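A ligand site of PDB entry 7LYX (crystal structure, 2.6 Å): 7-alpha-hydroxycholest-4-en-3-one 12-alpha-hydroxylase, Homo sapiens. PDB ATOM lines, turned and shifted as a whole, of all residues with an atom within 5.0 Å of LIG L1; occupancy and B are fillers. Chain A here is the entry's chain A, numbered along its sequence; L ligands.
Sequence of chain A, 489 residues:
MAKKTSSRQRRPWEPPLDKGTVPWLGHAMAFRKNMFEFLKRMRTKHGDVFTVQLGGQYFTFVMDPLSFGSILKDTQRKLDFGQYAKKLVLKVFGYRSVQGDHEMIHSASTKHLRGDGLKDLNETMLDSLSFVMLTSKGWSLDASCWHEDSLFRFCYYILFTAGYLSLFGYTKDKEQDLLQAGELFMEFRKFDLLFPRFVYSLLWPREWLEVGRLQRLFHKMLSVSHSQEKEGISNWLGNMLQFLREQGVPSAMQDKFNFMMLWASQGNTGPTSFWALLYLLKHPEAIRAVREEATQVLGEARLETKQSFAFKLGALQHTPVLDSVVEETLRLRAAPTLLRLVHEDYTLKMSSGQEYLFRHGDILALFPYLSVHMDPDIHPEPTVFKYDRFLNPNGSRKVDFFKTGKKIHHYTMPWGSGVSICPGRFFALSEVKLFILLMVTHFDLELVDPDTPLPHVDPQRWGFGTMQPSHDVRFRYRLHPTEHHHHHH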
ATOM      1  N   PHE A  81      12.940 -22.861  30.812  1.00  0.00           N
ATOM      2  CA  PHE A  81      13.259 -24.178  30.280  1.00  0.00           C
ATOM      3  C   PHE A  81      13.999 -25.036  31.310  1.00  0.00           C
ATOM      4  O   PHE A  81      13.763 -26.240  31.390  1.00  0.00           O
ATOM      5  CB  PHE A  81      14.102 -24.010  29.006  1.00  0.00           C
ATOM      6  CG  PHE A  81      14.891 -25.233  28.636  1.00  0.00           C
ATOM      7  CD1 PHE A  81      14.362 -26.193  27.797  1.00  0.00           C
ATOM      8  CD2 PHE A  81      16.180 -25.415  29.112  1.00  0.00           C
ATOM      9  CE1 PHE A  81      15.086 -27.318  27.456  1.00  0.00           C
ATOM     10  CE2 PHE A  81      16.918 -26.537  28.780  1.00  0.00           C
ATOM     11  CZ  PHE A  81      16.367 -27.492  27.942  1.00  0.00           C
ATOM     12  N   HIS A 102      23.376 -23.480  34.951  1.00  0.00           N
ATOM     13  CA  HIS A 102      22.757 -23.114  33.677  1.00  0.00           C
ATOM     14  C   HIS A 102      23.536 -22.011  32.989  1.00  0.00           C
ATOM     15  O   HIS A 102      23.750 -22.056  31.764  1.00  0.00           O
ATOM     16  CB  HIS A 102      21.309 -22.671  33.887  1.00  0.00           C
ATOM     17  CG  HIS A 102      20.687 -22.099  32.641  1.00  0.00           C
ATOM     18  ND1 HIS A 102      20.991 -20.846  32.163  1.00  0.00           N
ATOM     19  CD2 HIS A 102      19.782 -22.635  31.780  1.00  0.00           C
ATOM     20  CE1 HIS A 102      20.305 -20.623  31.054  1.00  0.00           C
ATOM     21  NE2 HIS A 102      19.566 -21.684  30.805  1.00  0.00           N
ATOM     22  N   ILE A 105      27.174 -23.117  31.719  1.00  0.00           N
ATOM     23  CA  ILE A 105      27.189 -23.835  30.451  1.00  0.00           C
ATOM     24  C   ILE A 105      27.187 -22.844  29.295  1.00  0.00           C
ATOM     25  O   ILE A 105      28.011 -22.926  28.372  1.00  0.00           O
ATOM     26  CB  ILE A 105      25.996 -24.808  30.368  1.00  0.00           C
ATOM     27  CG1 ILE A 105      26.135 -25.911  31.429  1.00  0.00           C
ATOM     28  CG2 ILE A 105      25.907 -25.425  28.985  1.00  0.00           C
ATOM     29  CD1 ILE A 105      24.814 -26.498  31.881  1.00  0.00           C
ATOM     30  N   HIS A 106      26.280 -21.872  29.337  1.00  0.00           N
ATOM     31  CA  HIS A 106      26.166 -20.909  28.243  1.00  0.00           C
ATOM     32  C   HIS A 106      27.431 -20.071  28.121  1.00  0.00           C
ATOM     33  O   HIS A 106      27.950 -19.878  27.017  1.00  0.00           O
ATOM     34  CB  HIS A 106      24.940 -20.025  28.460  1.00  0.00           C
ATOM     35  CG  HIS A 106      23.657 -20.684  28.044  1.00  0.00           C
ATOM     36  ND1 HIS A 106      23.238 -20.743  26.734  1.00  0.00           N
ATOM     37  CD2 HIS A 106      22.716 -21.330  28.764  1.00  0.00           C
ATOM     38  CE1 HIS A 106      22.085 -21.383  26.661  1.00  0.00           C
ATOM     39  NE2 HIS A 106      21.746 -21.753  27.885  1.00  0.00           N
ATOM     40  N   LEU A 113      32.795 -22.323  22.218  1.00  0.00           N
ATOM     41  CA  LEU A 113      32.181 -22.996  21.076  1.00  0.00           C
ATOM     42  C   LEU A 113      31.680 -21.980  20.062  1.00  0.00           C
ATOM     43  O   LEU A 113      30.735 -22.242  19.316  1.00  0.00           O
ATOM     44  CB  LEU A 113      31.053 -23.915  21.530  1.00  0.00           C
ATOM     45  CG  LEU A 113      31.451 -25.030  22.500  1.00  0.00           C
ATOM     46  CD1 LEU A 113      30.232 -25.875  22.864  1.00  0.00           C
ATOM     47  CD2 LEU A 113      32.554 -25.909  21.913  1.00  0.00           C
ATOM     48  N   LEU A 167      36.559 -33.131  22.318  1.00  0.00           N
ATOM     49  CA  LEU A 167      36.020 -32.449  23.496  1.00  0.00           C
ATOM     50  C   LEU A 167      36.566 -33.002  24.803  1.00  0.00           C
ATOM     51  O   LEU A 167      36.987 -32.240  25.666  1.00  0.00           O
ATOM     52  CB  LEU A 167      34.484 -32.545  23.497  1.00  0.00           C
ATOM     53  CG  LEU A 167      33.756 -31.671  22.476  1.00  0.00           C
ATOM     54  CD1 LEU A 167      32.252 -31.870  22.523  1.00  0.00           C
ATOM     55  CD2 LEU A 167      34.103 -30.196  22.687  1.00  0.00           C
ATOM     56  N   TRP A 236      35.989 -25.874  26.654  1.00  0.00           N
ATOM     57  CA  TRP A 236      34.578 -25.939  27.015  1.00  0.00           C
ATOM     58  C   TRP A 236      34.361 -26.849  28.219  1.00  0.00           C
ATOM     59  O   TRP A 236      33.693 -26.463  29.184  1.00  0.00           O
ATOM     60  CB  TRP A 236      33.762 -26.423  25.808  1.00  0.00           C
ATOM     61  CG  TRP A 236      32.301 -26.594  26.073  1.00  0.00           C
ATOM     62  CD1 TRP A 236      31.398 -25.620  26.359  1.00  0.00           C
ATOM     63  CD2 TRP A 236      31.584 -27.829  26.061  1.00  0.00           C
ATOM     64  NE1 TRP A 236      30.149 -26.165  26.527  1.00  0.00           N
ATOM     65  CE2 TRP A 236      30.231 -27.523  26.355  1.00  0.00           C
ATOM     66  CE3 TRP A 236      31.932 -29.163  25.832  1.00  0.00           C
ATOM     67  CZ2 TRP A 236      29.244 -28.506  26.425  1.00  0.00           C
ATOM     68  CZ3 TRP A 236      30.957 -30.137  25.904  1.00  0.00           C
ATOM     69  CH2 TRP A 236      29.633 -29.799  26.199  1.00  0.00           C
ATOM     70  N   MET A 261      27.000 -34.421  29.529  1.00  0.00           N
ATOM     71  CA  MET A 261      27.489 -33.591  28.432  1.00  0.00           C
ATOM     72  C   MET A 261      27.990 -34.440  27.271  1.00  0.00           C
ATOM     73  O   MET A 261      27.920 -33.992  26.134  1.00  0.00           O
ATOM     74  CB  MET A 261      28.620 -32.666  28.850  1.00  0.00           C
ATOM     75  CG  MET A 261      28.203 -31.487  29.705  1.00  0.00           C
ATOM     76  SD  MET A 261      26.997 -30.443  28.841  1.00  0.00           S
ATOM     77  CE  MET A 261      25.543 -30.758  29.838  1.00  0.00           C
ATOM     78  N   ALA A 264      24.902 -35.058  25.389  1.00  0.00           N
ATOM     79  CA  ALA A 264      24.356 -33.831  24.825  1.00  0.00           C
ATOM     80  C   ALA A 264      25.130 -33.408  23.588  1.00  0.00           C
ATOM     81  O   ALA A 264      24.547 -32.894  22.628  1.00  0.00           O
ATOM     82  CB  ALA A 264      24.375 -32.712  25.873  1.00  0.00           C
ATOM     83  N   SER A 265      26.443 -33.618  23.566  1.00  0.00           N
ATOM     84  CA  SER A 265      27.271 -33.144  22.473  1.00  0.00           C
ATOM     85  C   SER A 265      27.405 -34.167  21.350  1.00  0.00           C
ATOM     86  O   SER A 265      27.740 -33.776  20.226  1.00  0.00           O
ATOM     87  CB  SER A 265      28.666 -32.792  22.990  1.00  0.00           C
ATOM     88  OG  SER A 265      29.263 -33.898  23.633  1.00  0.00           O
ATOM     89  N   ASN A 268      23.155 -35.986  18.711  1.00  0.00           N
ATOM     90  CA  ASN A 268      22.466 -35.614  17.481  1.00  0.00           C
ATOM     91  C   ASN A 268      23.388 -35.315  16.328  1.00  0.00           C
ATOM     92  O   ASN A 268      22.968 -35.479  15.170  1.00  0.00           O
ATOM     93  CB  ASN A 268      21.572 -34.383  17.733  1.00  0.00           C
ATOM     94  CG  ASN A 268      20.523 -34.648  18.775  1.00  0.00           C
ATOM     95  OD1 ASN A 268      19.738 -35.586  18.660  1.00  0.00           O
ATOM     96  ND2 ASN A 268      20.489 -33.806  19.798  1.00  0.00           N
ATOM     97  N   THR A 269      24.623 -34.898  16.586  1.00  0.00           N
ATOM     98  CA  THR A 269      25.521 -34.530  15.500  1.00  0.00           C
ATOM     99  C   THR A 269      25.680 -35.684  14.504  1.00  0.00           C
ATOM    100  O   THR A 269      25.592 -35.481  13.281  1.00  0.00           O
ATOM    101  CB  THR A 269      26.864 -34.084  16.079  1.00  0.00           C
ATOM    102  OG1 THR A 269      27.584 -33.317  15.098  1.00  0.00           O
ATOM    103  CG2 THR A 269      27.706 -35.268  16.527  1.00  0.00           C
ATOM    104  N   THR A 272      22.414 -36.510  12.447  1.00  0.00           N
ATOM    105  CA  THR A 272      22.176 -35.462  11.475  1.00  0.00           C
ATOM    106  C   THR A 272      23.109 -35.596  10.274  1.00  0.00           C
ATOM    107  O   THR A 272      22.718 -35.265   9.145  1.00  0.00           O
ATOM    108  CB  THR A 272      22.369 -34.088  12.123  1.00  0.00           C
ATOM    109  OG1 THR A 272      21.377 -33.884  13.124  1.00  0.00           O
ATOM    110  CG2 THR A 272      22.275 -32.987  11.067  1.00  0.00           C
ATOM    111  N   LEU A 330      18.019 -30.552   8.599  1.00  0.00           N
ATOM    112  CA  LEU A 330      17.483 -30.276   9.928  1.00  0.00           C
ATOM    113  C   LEU A 330      15.990 -29.960   9.865  1.00  0.00           C
ATOM    114  O   LEU A 330      15.240 -30.325  10.783  1.00  0.00           O
ATOM    115  CB  LEU A 330      18.230 -29.112  10.567  1.00  0.00           C
ATOM    116  CG  LEU A 330      19.657 -29.383  11.060  1.00  0.00           C
ATOM    117  CD1 LEU A 330      20.371 -28.075  11.345  1.00  0.00           C
ATOM    118  CD2 LEU A 330      19.612 -30.265  12.291  1.00  0.00           C
ATOM    119  N   ALA A 334      15.089 -32.708  12.241  1.00  0.00           N
ATOM    120  CA  ALA A 334      15.213 -32.180  13.607  1.00  0.00           C
ATOM    121  C   ALA A 334      13.809 -31.886  14.114  1.00  0.00           C
ATOM    122  O   ALA A 334      13.164 -30.928  13.682  1.00  0.00           O
ATOM    123  CB  ALA A 334      16.082 -30.919  13.624  1.00  0.00           C
ATOM    124  N   PRO A 336      12.451 -31.513  17.658  1.00  0.00           N
ATOM    125  CA  PRO A 336      12.423 -31.381  19.117  1.00  0.00           C
ATOM    126  C   PRO A 336      11.130 -30.760  19.620  1.00  0.00           C
ATOM    127  O   PRO A 336      10.365 -30.138  18.881  1.00  0.00           O
ATOM    128  CB  PRO A 336      13.606 -30.457  19.398  1.00  0.00           C
ATOM    129  CG  PRO A 336      13.688 -29.578  18.175  1.00  0.00           C
ATOM    130  CD  PRO A 336      13.230 -30.445  17.011  1.00  0.00           C
ATOM    131  N   LEU A 338       9.874 -27.956  22.436  1.00  0.00           N
ATOM    132  CA  LEU A 338      10.339 -26.791  23.183  1.00  0.00           C
ATOM    133  C   LEU A 338       9.469 -26.656  24.428  1.00  0.00           C
ATOM    134  O   LEU A 338       8.304 -26.272  24.334  1.00  0.00           O
ATOM    135  CB  LEU A 338      10.289 -25.527  22.329  1.00  0.00           C
ATOM    136  CG  LEU A 338      11.515 -25.281  21.445  1.00  0.00           C
ATOM    137  CD1 LEU A 338      11.962 -26.584  20.783  1.00  0.00           C
ATOM    138  CD2 LEU A 338      11.221 -24.219  20.396  1.00  0.00           C
ATOM    139  N   ARG A 340       8.699 -25.318  28.404  1.00  0.00           N
ATOM    140  CA  ARG A 340       8.908 -24.254  29.369  1.00  0.00           C
ATOM    141  C   ARG A 340       7.952 -24.451  30.522  1.00  0.00           C
ATOM    142  O   ARG A 340       6.742 -24.643  30.310  1.00  0.00           O
ATOM    143  CB  ARG A 340       8.683 -22.867  28.733  1.00  0.00           C
ATOM    144  CG  ARG A 340       9.292 -22.686  27.371  1.00  0.00           C
ATOM    145  CD  ARG A 340      10.772 -22.376  27.481  1.00  0.00           C
ATOM    146  NE  ARG A 340      11.376 -22.102  26.184  1.00  0.00           N
ATOM    147  CZ  ARG A 340      12.024 -23.010  25.464  1.00  0.00           C
ATOM    148  NH1 ARG A 340      12.162 -24.258  25.905  1.00  0.00           N
ATOM    149  NH2 ARG A 340      12.550 -22.674  24.288  1.00  0.00           N
ATOM    150  N   PRO A 414      15.458 -25.911  14.435  1.00  0.00           N
ATOM    151  CA  PRO A 414      16.169 -27.097  14.936  1.00  0.00           C
ATOM    152  C   PRO A 414      16.860 -26.876  16.263  1.00  0.00           C
ATOM    153  O   PRO A 414      17.054 -27.853  16.995  1.00  0.00           O
ATOM    154  CB  PRO A 414      17.204 -27.382  13.831  1.00  0.00           C
ATOM    155  CG  PRO A 414      17.476 -26.026  13.230  1.00  0.00           C
ATOM    156  CD  PRO A 414      16.196 -25.214  13.373  1.00  0.00           C
ATOM    157  N   TRP A 415      17.194 -25.629  16.614  1.00  0.00           N
ATOM    158  CA  TRP A 415      17.923 -25.334  17.845  1.00  0.00           C
ATOM    159  C   TRP A 415      17.054 -24.729  18.941  1.00  0.00           C
ATOM    160  O   TRP A 415      17.476 -24.685  20.097  1.00  0.00           O
ATOM    161  CB  TRP A 415      19.072 -24.353  17.563  1.00  0.00           C
ATOM    162  CG  TRP A 415      19.797 -24.635  16.294  1.00  0.00           C
ATOM    163  CD1 TRP A 415      19.795 -23.872  15.150  1.00  0.00           C
ATOM    164  CD2 TRP A 415      20.655 -25.742  16.019  1.00  0.00           C
ATOM    165  NE1 TRP A 415      20.590 -24.449  14.198  1.00  0.00           N
ATOM    166  CE2 TRP A 415      21.136 -25.598  14.704  1.00  0.00           C
ATOM    167  CE3 TRP A 415      21.070 -26.855  16.768  1.00  0.00           C
ATOM    168  CZ2 TRP A 415      21.995 -26.514  14.119  1.00  0.00           C
ATOM    169  CZ3 TRP A 415      21.927 -27.758  16.184  1.00  0.00           C
ATOM    170  CH2 TRP A 415      22.385 -27.588  14.876  1.00  0.00           C
ATOM    171  N   GLY A 416      15.850 -24.252  18.597  1.00  0.00           N
ATOM    172  CA  GLY A 416      15.004 -23.588  19.558  1.00  0.00           C
ATOM    173  C   GLY A 416      15.151 -22.088  19.506  1.00  0.00           C
ATOM    174  O   GLY A 416      15.500 -21.531  18.466  1.00  0.00           O
ATOM    175  N   SER A 417      14.890 -21.388  20.599  1.00  0.00           N
ATOM    176  CA  SER A 417      15.088 -19.946  20.629  1.00  0.00           C
ATOM    177  C   SER A 417      15.111 -19.514  22.088  1.00  0.00           C
ATOM    178  O   SER A 417      14.965 -20.340  22.990  1.00  0.00           O
ATOM    179  CB  SER A 417      14.013 -19.270  19.762  1.00  0.00           C
ATOM    180  OG  SER A 417      14.208 -17.864  19.695  1.00  0.00           O
ATOM    181  N   SER A 420      17.701 -20.372  25.956  1.00  0.00           N
ATOM    182  CA  SER A 420      18.001 -21.795  26.057  1.00  0.00           C
ATOM    183  C   SER A 420      18.316 -22.412  24.700  1.00  0.00           C
ATOM    184  O   SER A 420      18.328 -23.651  24.580  1.00  0.00           O
ATOM    185  CB  SER A 420      16.845 -22.539  26.703  1.00  0.00           C
ATOM    186  OG  SER A 420      15.666 -22.439  25.919  1.00  0.00           O
ATOM    187  N   ILE A 421      18.554 -21.598  23.676  1.00  0.00           N
ATOM    188  CA  ILE A 421      18.875 -22.129  22.357  1.00  0.00           C
ATOM    189  C   ILE A 421      20.205 -22.855  22.410  1.00  0.00           C
ATOM    190  O   ILE A 421      21.129 -22.439  23.125  1.00  0.00           O
ATOM    191  CB  ILE A 421      18.889 -20.993  21.308  1.00  0.00           C
ATOM    192  CG1 ILE A 421      19.051 -21.565  19.911  1.00  0.00           C
ATOM    193  CG2 ILE A 421      20.001 -20.000  21.623  1.00  0.00           C
ATOM    194  CD1 ILE A 421      18.589 -20.623  18.816  1.00  0.00           C
ATOM    195  N   CYS A 422      20.299 -23.945  21.667  1.00  0.00           N
ATOM    196  CA  CYS A 422      21.433 -24.846  21.773  1.00  0.00           C
ATOM    197  C   CYS A 422      22.767 -24.119  21.758  1.00  0.00           C
ATOM    198  O   CYS A 422      23.146 -23.537  20.744  1.00  0.00           O
ATOM    199  CB  CYS A 422      21.394 -25.861  20.628  1.00  0.00           C
ATOM    200  SG  CYS A 422      22.897 -26.817  20.478  1.00  0.00           S
ATOM    201  N   PRO A 423      23.518 -24.156  22.868  1.00  0.00           N
ATOM    202  CA  PRO A 423      24.809 -23.456  22.896  1.00  0.00           C
ATOM    203  C   PRO A 423      25.906 -24.159  22.110  1.00  0.00           C
ATOM    204  O   PRO A 423      27.021 -23.624  22.036  1.00  0.00           O
ATOM    205  CB  PRO A 423      25.161 -23.390  24.386  1.00  0.00           C
ATOM    206  CG  PRO A 423      24.384 -24.494  25.027  1.00  0.00           C
ATOM    207  CD  PRO A 423      23.206 -24.814  24.150  1.00  0.00           C
ATOM    208  N   GLY A 424      25.639 -25.307  21.503  1.00  0.00           N
ATOM    209  CA  GLY A 424      26.641 -26.007  20.725  1.00  0.00           C
ATOM    210  C   GLY A 424      26.267 -26.125  19.271  1.00  0.00           C
ATOM    211  O   GLY A 424      26.806 -26.961  18.545  1.00  0.00           O
ATOM    212  N   PHE A 427      29.245 -25.481  16.795  1.00  0.00           N
ATOM    213  CA  PHE A 427      30.124 -26.642  16.713  1.00  0.00           C
ATOM    214  C   PHE A 427      29.449 -27.776  15.944  1.00  0.00           C
ATOM    215  O   PHE A 427      30.038 -28.343  15.022  1.00  0.00           O
ATOM    216  CB  PHE A 427      30.504 -27.115  18.114  1.00  0.00           C
ATOM    217  CG  PHE A 427      31.484 -28.255  18.120  1.00  0.00           C
ATOM    218  CD1 PHE A 427      32.683 -28.148  17.446  1.00  0.00           C
ATOM    219  CD2 PHE A 427      31.192 -29.428  18.780  1.00  0.00           C
ATOM    220  CE1 PHE A 427      33.592 -29.183  17.445  1.00  0.00           C
ATOM    221  CE2 PHE A 427      32.093 -30.478  18.783  1.00  0.00           C
ATOM    222  CZ  PHE A 427      33.291 -30.356  18.108  1.00  0.00           C
ATOM    223  N   ALA A 428      28.218 -28.132  16.339  1.00  0.00           N
ATOM    224  CA  ALA A 428      27.487 -29.173  15.618  1.00  0.00           C
ATOM    225  C   ALA A 428      27.520 -28.935  14.122  1.00  0.00           C
ATOM    226  O   ALA A 428      27.685 -29.867  13.333  1.00  0.00           O
ATOM    227  CB  ALA A 428      26.046 -29.233  16.121  1.00  0.00           C
ATOM    228  N   GLU A 431      30.969 -29.559  12.878  1.00  0.00           N
ATOM    229  CA  GLU A 431      31.069 -31.006  12.910  1.00  0.00           C
ATOM    230  C   GLU A 431      30.468 -31.636  11.654  1.00  0.00           C
ATOM    231  O   GLU A 431      31.128 -32.399  10.951  1.00  0.00           O
ATOM    232  CB  GLU A 431      30.371 -31.556  14.162  1.00  0.00           C
ATOM    233  CG  GLU A 431      31.100 -31.323  15.480  1.00  0.00           C
ATOM    234  CD  GLU A 431      30.676 -32.324  16.552  1.00  0.00           C
ATOM    235  OE1 GLU A 431      31.286 -33.410  16.630  1.00  0.00           O
ATOM    236  OE2 GLU A 431      29.735 -32.015  17.311  1.00  0.00           O
ATOM    237  N   THR A 466      17.225 -34.814  16.962  1.00  0.00           N
ATOM    238  CA  THR A 466      17.276 -35.285  15.590  1.00  0.00           C
ATOM    239  C   THR A 466      16.733 -36.706  15.524  1.00  0.00           C
ATOM    240  O   THR A 466      17.147 -37.577  16.291  1.00  0.00           O
ATOM    241  CB  THR A 466      18.698 -35.235  15.041  1.00  0.00           C
ATOM    242  OG1 THR A 466      19.134 -33.878  14.962  1.00  0.00           O
ATOM    243  CG2 THR A 466      18.741 -35.878  13.651  1.00  0.00           C
HETATM  244  C1  LIG L   1      19.749 -27.449  23.910  1.00  0.00           C
HETATM  245  C2  LIG L   1      19.158 -29.220  19.422  1.00  0.00           C
HETATM  246  C3  LIG L   1      23.860 -30.396  19.272  1.00  0.00           C
HETATM  247  C4  LIG L   1      24.401 -28.873  23.856  1.00  0.00           C
HETATM  248  C5  LIG L   1      19.175 -27.825  22.713  1.00  0.00           C
HETATM  249  C6  LIG L   1      17.777 -27.664  22.336  1.00  0.00           C
HETATM  250  C7  LIG L   1      17.617 -28.153  21.105  1.00  0.00           C
HETATM  251  C8  LIG L   1      18.898 -28.640  20.637  1.00  0.00           C
HETATM  252  C9  LIG L   1      16.301 -28.184  20.293  1.00  0.00           C
HETATM  253  C10 LIG L   1      16.662 -27.026  23.218  1.00  0.00           C
HETATM  254  C11 LIG L   1      16.396 -25.608  22.727  1.00  0.00           C
HETATM  255  C12 LIG L   1      15.387 -24.894  23.599  1.00  0.00           C
HETATM  256  O1  LIG L   1      15.170 -23.675  23.352  1.00  0.00           O
HETATM  257  O2  LIG L   1      14.821 -25.521  24.517  1.00  0.00           O
HETATM  258  C13 LIG L   1      20.382 -29.706  19.001  1.00  0.00           C
HETATM  259  C14 LIG L   1      20.613 -30.376  17.742  1.00  0.00           C
HETATM  260  C15 LIG L   1      21.911 -30.722  17.695  1.00  0.00           C
HETATM  261  C16 LIG L   1      22.541 -30.261  18.919  1.00  0.00           C
HETATM  262  C17 LIG L   1      19.507 -30.638  16.687  1.00  0.00           C
HETATM  263  C18 LIG L   1      22.676 -31.447  16.549  1.00  0.00           C
HETATM  264  C19 LIG L   1      22.148 -31.568  15.326  1.00  0.00           C
HETATM  265  C20 LIG L   1      24.425 -30.049  20.491  1.00  0.00           C
HETATM  266  C21 LIG L   1      25.829 -30.124  20.829  1.00  0.00           C
HETATM  267  C22 LIG L   1      25.970 -29.716  22.096  1.00  0.00           C
HETATM  268  C23 LIG L   1      24.675 -29.352  22.599  1.00  0.00           C
HETATM  269  C24 LIG L   1      26.924 -30.637  19.857  1.00  0.00           C
HETATM  270  C25 LIG L   1      27.263 -29.588  22.958  1.00  0.00           C
HETATM  271  C26 LIG L   1      28.480 -29.626  22.415  1.00  0.00           C
HETATM  272  C27 LIG L   1      23.179 -28.407  24.301  1.00  0.00           C
HETATM  273  C28 LIG L   1      22.848 -28.027  25.656  1.00  0.00           C
HETATM  274  C29 LIG L   1      21.574 -27.621  25.674  1.00  0.00           C
HETATM  275  C30 LIG L   1      21.038 -27.751  24.325  1.00  0.00           C
HETATM  276  C31 LIG L   1      23.813 -28.066  26.861  1.00  0.00           C
HETATM  277  C32 LIG L   1      20.828 -27.150  26.949  1.00  0.00           C
HETATM  278  C33 LIG L   1      19.939 -25.921  26.740  1.00  0.00           C
HETATM  279  C34 LIG L   1      20.344 -24.896  27.772  1.00  0.00           C
HETATM  280  O3  LIG L   1      19.527 -24.593  28.672  1.00  0.00           O
HETATM  281  O4  LIG L   1      21.492 -24.400  27.686  1.00  0.00           O
HETATM  282  N1  LIG L   1      19.818 -28.429  21.649  1.00  0.00           N
HETATM  283  N2  LIG L   1      21.570 -29.649  19.696  1.00  0.00           N
HETATM  284  N3  LIG L   1      23.750 -29.570  21.598  1.00  0.00           N
HETATM  285  N4  LIG L   1      22.048 -28.230  23.523  1.00  0.00           N
HETATM  286 FE1  LIG L   1      21.779 -28.915  21.636  1.00  0.00          FE
HETATM  287  C1  LG2 L   2      14.218 -32.439  25.021  1.00  0.00           C
HETATM  288  C2  LG2 L   2      13.356 -33.446  24.283  1.00  0.00           C
HETATM  289  C3  LG2 L   2      21.677 -32.288  23.267  1.00  0.00           C
HETATM  290  C4  LG2 L   2      20.562 -32.885  23.766  1.00  0.00           C
HETATM  291  C5  LG2 L   2      19.513 -30.422  26.064  1.00  0.00           C
HETATM  292  C6  LG2 L   2      20.560 -31.445  27.965  1.00  0.00           C
HETATM  293  C7  LG2 L   2      19.731 -32.544  27.831  1.00  0.00           C
HETATM  294  C8  LG2 L   2      18.796 -32.579  26.808  1.00  0.00           C
HETATM  295  C9  LG2 L   2      18.681 -31.515  25.923  1.00  0.00           C
HETATM  296  C10 LG2 L   2      17.665 -31.511  24.771  1.00  0.00           C
HETATM  297  C11 LG2 L   2      15.356 -31.654  24.395  1.00  0.00           C
HETATM  298  C12 LG2 L   2      13.808 -32.339  26.393  1.00  0.00           C
HETATM  299  C13 LG2 L   2      12.401 -34.000  25.181  1.00  0.00           C
HETATM  300  C14 LG2 L   2      18.132 -32.479  23.677  1.00  0.00           C
HETATM  301  C15 LG2 L   2      19.962 -31.170  22.615  1.00  0.00           C
HETATM  302  C16 LG2 L   2      20.446 -30.395  27.080  1.00  0.00           C
HETATM  303  N1  LG2 L   2      19.523 -32.188  23.358  1.00  0.00           N
HETATM  304  N2  LG2 L   2      21.301 -31.248  22.560  1.00  0.00           N
HETATM  305  O1  LG2 L   2      16.433 -31.895  25.260  1.00  0.00           O
HETATM  306  S1  LG2 L   2      12.566 -33.345  26.653  1.00  0.00           S
HETATM  307 CL1  LG2 L   2      21.773 -31.367  29.276  1.00  0.00          CL
HETATM  308 CL2  LG2 L   2      17.746 -34.027  26.669  1.00  0.00          CL
HETATM  309 CL3  LG2 L   2      14.537 -31.281  27.635  1.00  0.00          CL
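A nitrogen (N2) of LG2 L2 is bound to an iron atom (FE1) of LIG L1.
The backbone carbonyl oxygen of Ser 417 sits close to an oxygen (O1) of LIG L1. CE2 of Phe 81 touches O3 of LIG L1, 3.3 Å away. His 102 touches LIG L1. Ile 105 touches LIG L1 (CG2 to C31, 3.98 Å). Trp 236 touches LIG L1. Ala 264 touches LIG L1 (O to C22, 3.5 Å). Ser 265 touches LIG L1. Asn 268 touches LIG L1. N of Thr 269 touches C18 of LIG L1, 3.96 Å away. OG1 of Thr 272 touches C19 of LIG L1 (3.3 Å). CB of Pro 336 touches C9 of LIG L1, at 3.6 Å. Pro 414 touches LIG L1 (O to C9, 3.4 Å). Trp 415 touches LIG L1 (O to C11, 3.0 Å). Gly 416 touches LIG L1 (CA to O1, 3.8 Å). Ile 421 touches LIG L1 (N to O1, 3.98 Å). Pro 423 touches LIG L1 (CD to C28, 3.6 Å). O of Gly 424 touches C24 of LIG L1, at 3.9 Å. Thr 466 touches LIG L1. 22 residues have an atom within 4 Å of LIG L1: Phe 81, His 102, Ile 105, His 106, Trp 236, Ala 264, Ser 265, Asn 268, Thr 269, Thr 272, Pro 336, Arg 340, Pro 414, Trp 415, Gly 416, Ser 417, Ser 420, Ile 421, Cys 422, Pro 423, Gly 424 and Thr 466. The nearest printed residue that does not touch LIG L1 is Ala 428 (4.01 Å).
SG of Cys 422 is bound to FE1 of LIG L1 (2.6 Å). O1 of LIG L1 lies within hydrogen-bond range of OG of Ser 420. NH2 of Arg 340 lies within salt-bridge range of O1 of LIG L1, at 3.0 Å. A ring nitrogen (NE2) of His 106 is in hydrogen-bond range of an oxygen (O4) of LIG L1 (2.7 Å).
SG of Cys 422 sits close to N of Gly 424, 3.3 Å away. The backbone carbonyl oxygen (O) of Trp 415 sits at hydrogen-bond distance from the backbone NH (N) of Cys 422 (3.3 Å). The side-chain hydroxyl (OG1) of Thr 466 is in hydrogen-bond range of the side-chain hydroxyl (OG1) of Thr 272. OD1 of Asn 268 sits at hydrogen-bond distance from N of Thr 466 (3.1 Å). O of Met 261 sits at hydrogen-bond distance from OG of Ser 265, at 2.8 Å. The side-chain hydroxyl (OG1) of Thr 272 lies within hydrogen-bond range of the backbone carbonyl oxygen (O) of Asn 268 (3.0 Å). The side-chain carboxylate of Glu 431 is in hydrogen-bond range of the side-chain hydroxyl of Thr 269 (3.3 Å).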
